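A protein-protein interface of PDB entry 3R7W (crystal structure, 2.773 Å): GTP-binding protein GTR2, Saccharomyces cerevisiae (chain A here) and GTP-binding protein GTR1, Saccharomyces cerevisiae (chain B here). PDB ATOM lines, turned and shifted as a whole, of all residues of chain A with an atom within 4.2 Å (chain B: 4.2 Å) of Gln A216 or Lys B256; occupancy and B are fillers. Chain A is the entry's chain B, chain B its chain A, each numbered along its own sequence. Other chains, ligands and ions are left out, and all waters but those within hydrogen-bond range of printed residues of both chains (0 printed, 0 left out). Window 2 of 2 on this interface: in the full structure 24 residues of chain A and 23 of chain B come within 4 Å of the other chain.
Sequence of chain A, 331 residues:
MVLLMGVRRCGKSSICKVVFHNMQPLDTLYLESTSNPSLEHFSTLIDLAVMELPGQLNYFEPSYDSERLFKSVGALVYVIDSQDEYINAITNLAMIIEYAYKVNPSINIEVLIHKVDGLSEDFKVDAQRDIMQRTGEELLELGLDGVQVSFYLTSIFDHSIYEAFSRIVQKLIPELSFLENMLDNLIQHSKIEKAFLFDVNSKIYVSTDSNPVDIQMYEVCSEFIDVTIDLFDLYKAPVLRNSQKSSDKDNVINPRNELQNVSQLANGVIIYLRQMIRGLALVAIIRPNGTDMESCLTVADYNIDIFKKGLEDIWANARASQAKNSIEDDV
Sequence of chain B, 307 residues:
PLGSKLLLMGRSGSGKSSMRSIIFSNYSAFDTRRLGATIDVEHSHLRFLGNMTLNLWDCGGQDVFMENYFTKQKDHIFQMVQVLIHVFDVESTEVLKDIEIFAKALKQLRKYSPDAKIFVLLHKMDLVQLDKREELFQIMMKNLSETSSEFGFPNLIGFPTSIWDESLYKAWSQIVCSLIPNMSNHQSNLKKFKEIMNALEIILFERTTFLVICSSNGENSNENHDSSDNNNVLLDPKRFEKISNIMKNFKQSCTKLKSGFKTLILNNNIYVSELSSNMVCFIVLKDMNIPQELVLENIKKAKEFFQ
The side-chain amino group of Lys B256 lies within salt-bridge range of the side-chain carboxylate of Glu A219 (3.3 Å).
The side-chain carboxylate (OE1) of Glu A223 sits at hydrogen-bond distance from the side-chain hydroxyl (OG) of Ser B253 (3.0 Å).
Hydrophobic or aromatic side chains of chain B within 4 Å of the printed part of chain A: Leu B257.
Hydrophobic or aromatic side chains of chain A within 4 Å of the printed part of chain B: Met A217 and Val A220.
Among the printed residues, 7 pairs touch across the chains.
Lys B256 touches Gln A216.
Leu B257 touches Met A217.
Val A220 touches Lys B256 (CG2 to CB, 3.8 Å).
CD1 of Leu B257 touches CG1 of Val A220, 3.7 Å away.
Lys B256 touches Glu A223.
Of chain B, only Lys B256 (3.3 Å) comes within 4 Å of Gln A216.
Of chain A, only Gln A216 (3.3 Å), Glu A219 (2.8 Å), Val A220 (3.8 Å) and Glu A223 (3.4 Å) come within 4 Å of Lys B256.
Of the printed residues of chain B, Val A220 touches Lys B256 and Leu B257.
Of the printed residues of chain B, Glu A219 touches Lys B256 (2.8 Å).
Of the printed residues of chain B, Met A217 touches Leu B257 (3.4 Å).
Printed residues of chain B within 4 Å of Glu A223: Ser B253 (3.0 Å) and Lys B256 (3.4 Å).
Of the printed residues of chain A, Leu B257 touches Met A217 (3.4 Å) and Val A220 (3.7 Å).
The nearest printed residue of chain A that does not touch Lys B256 is Met A217 (5.2 Å).
The nearest printed residue of chain B that does not touch Glu A223 is Cys B254 (5.9 Å).
The side-chain carboxylate (OD1) of Asp A214 lies close to the backbone NH (N) of Gln A216 (3.5 Å).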
ATOM      1  N   ASP A 214      13.281  -1.275  16.814  1.00  0.00           N
ATOM      2  CA  ASP A 214      13.761  -0.017  17.409  1.00  0.00           C
ATOM      3  C   ASP A 214      13.923   1.036  16.307  1.00  0.00           C
ATOM      4  O   ASP A 214      14.775   0.895  15.419  1.00  0.00           O
ATOM      5  CB  ASP A 214      15.078  -0.185  18.188  1.00  0.00           C
ATOM      6  CG  ASP A 214      15.699   1.158  18.590  1.00  0.00           C
ATOM      7  OD1 ASP A 214      14.938   2.078  18.984  1.00  0.00           O
ATOM      8  OD2 ASP A 214      16.944   1.291  18.502  1.00  0.00           O
ATOM      9  N   ILE A 215      13.106   2.088  16.376  1.00  0.00           N
ATOM     10  CA  ILE A 215      13.018   3.067  15.292  1.00  0.00           C
ATOM     11  C   ILE A 215      14.358   3.786  15.013  1.00  0.00           C
ATOM     12  O   ILE A 215      14.599   4.279  13.898  1.00  0.00           O
ATOM     13  CB  ILE A 215      11.863   4.093  15.540  1.00  0.00           C
ATOM     14  CG1 ILE A 215      11.355   4.671  14.208  1.00  0.00           C
ATOM     15  CG2 ILE A 215      12.290   5.178  16.546  1.00  0.00           C
ATOM     16  CD1 ILE A 215      10.459   5.904  14.338  1.00  0.00           C
ATOM     17  N   GLN A 216      15.231   3.820  16.017  1.00  0.00           N
ATOM     18  CA  GLN A 216      16.516   4.491  15.876  1.00  0.00           C
ATOM     19  C   GLN A 216      17.267   3.918  14.666  1.00  0.00           C
ATOM     20  O   GLN A 216      17.624   4.653  13.734  1.00  0.00           O
ATOM     21  CB  GLN A 216      17.333   4.340  17.164  1.00  0.00           C
ATOM     22  CG  GLN A 216      18.018   5.626  17.641  1.00  0.00           C
ATOM     23  CD  GLN A 216      17.033   6.699  18.116  1.00  0.00           C
ATOM     24  OE1 GLN A 216      15.824   6.464  18.201  1.00  0.00           O
ATOM     25  NE2 GLN A 216      17.556   7.885  18.428  1.00  0.00           N
ATOM     26  N   MET A 217      17.459   2.598  14.676  1.00  0.00           N
ATOM     27  CA  MET A 217      18.089   1.890  13.566  1.00  0.00           C
ATOM     28  C   MET A 217      17.357   2.123  12.259  1.00  0.00           C
ATOM     29  O   MET A 217      17.987   2.196  11.205  1.00  0.00           O
ATOM     30  CB  MET A 217      18.162   0.390  13.844  1.00  0.00           C
ATOM     31  CG  MET A 217      19.085   0.034  14.979  1.00  0.00           C
ATOM     32  SD  MET A 217      20.637   1.222  14.991  1.00  0.00           S
ATOM     33  CE  MET A 217      21.801   0.128  16.154  1.00  0.00           C
ATOM     34  N   TYR A 218      16.036   2.237  12.316  1.00  0.00           N
ATOM     35  CA  TYR A 218      15.289   2.536  11.099  1.00  0.00           C
ATOM     36  C   TYR A 218      15.600   3.941  10.546  1.00  0.00           C
ATOM     37  O   TYR A 218      15.662   4.142   9.322  1.00  0.00           O
ATOM     38  CB  TYR A 218      13.772   2.349  11.280  1.00  0.00           C
ATOM     39  CG  TYR A 218      13.008   2.903  10.101  1.00  0.00           C
ATOM     40  CD1 TYR A 218      12.867   2.168   8.933  1.00  0.00           C
ATOM     41  CD2 TYR A 218      12.480   4.185  10.136  1.00  0.00           C
ATOM     42  CE1 TYR A 218      12.199   2.685   7.845  1.00  0.00           C
ATOM     43  CE2 TYR A 218      11.821   4.718   9.046  1.00  0.00           C
ATOM     44  CZ  TYR A 218      11.680   3.962   7.910  1.00  0.00           C
ATOM     45  OH  TYR A 218      11.027   4.500   6.834  1.00  0.00           O
ATOM     46  N   GLU A 219      15.801   4.916  11.428  1.00  0.00           N
ATOM     47  CA  GLU A 219      15.981   6.288  10.954  1.00  0.00           C
ATOM     48  C   GLU A 219      17.327   6.461  10.272  1.00  0.00           C
ATOM     49  O   GLU A 219      17.416   6.936   9.126  1.00  0.00           O
ATOM     50  CB  GLU A 219      15.828   7.289  12.100  1.00  0.00           C
ATOM     51  CG  GLU A 219      14.542   8.107  12.032  1.00  0.00           C
ATOM     52  CD  GLU A 219      13.903   8.303  13.395  1.00  0.00           C
ATOM     53  OE1 GLU A 219      14.653   8.538  14.373  1.00  0.00           O
ATOM     54  OE2 GLU A 219      12.654   8.202  13.484  1.00  0.00           O
ATOM     55  N   VAL A 220      18.366   6.035  10.985  1.00  0.00           N
ATOM     56  CA  VAL A 220      19.732   6.128  10.492  1.00  0.00           C
ATOM     57  C   VAL A 220      19.789   5.628   9.051  1.00  0.00           C
ATOM     58  O   VAL A 220      20.100   6.392   8.120  1.00  0.00           O
ATOM     59  CB  VAL A 220      20.675   5.307  11.364  1.00  0.00           C
ATOM     60  CG1 VAL A 220      22.066   5.890  11.302  1.00  0.00           C
ATOM     61  CG2 VAL A 220      20.185   5.300  12.786  1.00  0.00           C
ATOM     62  N   GLU A 223      17.837   7.694   6.683  1.00  0.00           N
ATOM     63  CA  GLU A 223      18.427   9.010   6.523  1.00  0.00           C
ATOM     64  C   GLU A 223      19.680   8.866   5.685  1.00  0.00           C
ATOM     65  O   GLU A 223      20.032   9.764   4.907  1.00  0.00           O
ATOM     66  CB  GLU A 223      18.692   9.664   7.882  1.00  0.00           C
ATOM     67  CG  GLU A 223      17.526  10.568   8.339  1.00  0.00           C
ATOM     68  CD  GLU A 223      17.392  10.700   9.861  1.00  0.00           C
ATOM     69  OE1 GLU A 223      18.330  10.314  10.593  1.00  0.00           O
ATOM     70  OE2 GLU A 223      16.334  11.184  10.327  1.00  0.00           O
ATOM     71  N   SER B 253      22.054  13.043  12.352  1.00  0.00           N
ATOM     72  CA  SER B 253      21.520  11.694  12.272  1.00  0.00           C
ATOM     73  C   SER B 253      22.418  10.656  12.978  1.00  0.00           C
ATOM     74  O   SER B 253      21.904   9.792  13.689  1.00  0.00           O
ATOM     75  CB  SER B 253      21.271  11.329  10.805  1.00  0.00           C
ATOM     76  OG  SER B 253      21.259   9.929  10.621  1.00  0.00           O
ATOM     77  N   CYS B 254      23.744  10.753  12.800  1.00  0.00           N
ATOM     78  CA  CYS B 254      24.706   9.832  13.435  1.00  0.00           C
ATOM     79  C   CYS B 254      24.641   9.905  14.951  1.00  0.00           C
ATOM     80  O   CYS B 254      25.170   9.052  15.661  1.00  0.00           O
ATOM     81  CB  CYS B 254      26.140  10.095  12.985  1.00  0.00           C
ATOM     82  SG  CYS B 254      26.453   9.862  11.217  1.00  0.00           S
ATOM     83  N   THR B 255      23.985  10.938  15.440  1.00  0.00           N
ATOM     84  CA  THR B 255      23.658  11.066  16.845  1.00  0.00           C
ATOM     85  C   THR B 255      22.822   9.875  17.346  1.00  0.00           C
ATOM     86  O   THR B 255      22.893   9.500  18.517  1.00  0.00           O
ATOM     87  CB  THR B 255      22.902  12.387  17.035  1.00  0.00           C
ATOM     88  OG1 THR B 255      23.717  13.289  17.791  1.00  0.00           O
ATOM     89  CG2 THR B 255      21.504  12.181  17.660  1.00  0.00           C
ATOM     90  N   LYS B 256      22.046   9.282  16.437  1.00  0.00           N
ATOM     91  CA  LYS B 256      21.153   8.157  16.740  1.00  0.00           C
ATOM     92  C   LYS B 256      21.920   6.849  17.021  1.00  0.00           C
ATOM     93  O   LYS B 256      21.317   5.804  17.273  1.00  0.00           O
ATOM     94  CB  LYS B 256      20.156   7.938  15.578  1.00  0.00           C
ATOM     95  CG  LYS B 256      19.022   8.972  15.441  1.00  0.00           C
ATOM     96  CD  LYS B 256      18.580   9.132  13.969  1.00  0.00           C
ATOM     97  CE  LYS B 256      17.166   9.729  13.786  1.00  0.00           C
ATOM     98  NZ  LYS B 256      16.893  10.991  14.536  1.00  0.00           N
ATOM     99  N   LEU B 257      23.245   6.906  16.950  1.00  0.00           N
ATOM    100  CA  LEU B 257      24.080   5.741  17.199  1.00  0.00           C
ATOM    101  C   LEU B 257      25.150   6.161  18.196  1.00  0.00           C
ATOM    102  O   LEU B 257      26.102   5.416  18.488  1.00  0.00           O
ATOM    103  CB  LEU B 257      24.751   5.276  15.908  1.00  0.00           C
ATOM    104  CG  LEU B 257      23.900   4.763  14.757  1.00  0.00           C
ATOM    105  CD1 LEU B 257      24.761   4.595  13.515  1.00  0.00           C
ATOM    106  CD2 LEU B 257      23.267   3.446  15.162  1.00  0.00           C
ATOM    107  N   LYS B 258      25.010   7.391  18.679  1.00  0.00           N
ATOM    108  CA  LYS B 258      25.906   7.906  19.700  1.00  0.00           C
ATOM    109  C   LYS B 258      27.381   7.880  19.293  1.00  0.00           C
ATOM    110  O   LYS B 258      28.221   7.452  20.076  1.00  0.00           O
ATOM    111  CB  LYS B 258      25.699   7.112  20.988  1.00  0.00           C
ATOM    112  CG  LYS B 258      24.226   6.864  21.304  1.00  0.00           C
ATOM    113  CD  LYS B 258      24.055   6.394  22.741  1.00  0.00           C
ATOM    114  CE  LYS B 258      22.803   6.996  23.389  1.00  0.00           C
ATOM    115  NZ  LYS B 258      22.879   7.010  24.893  1.00  0.00           N
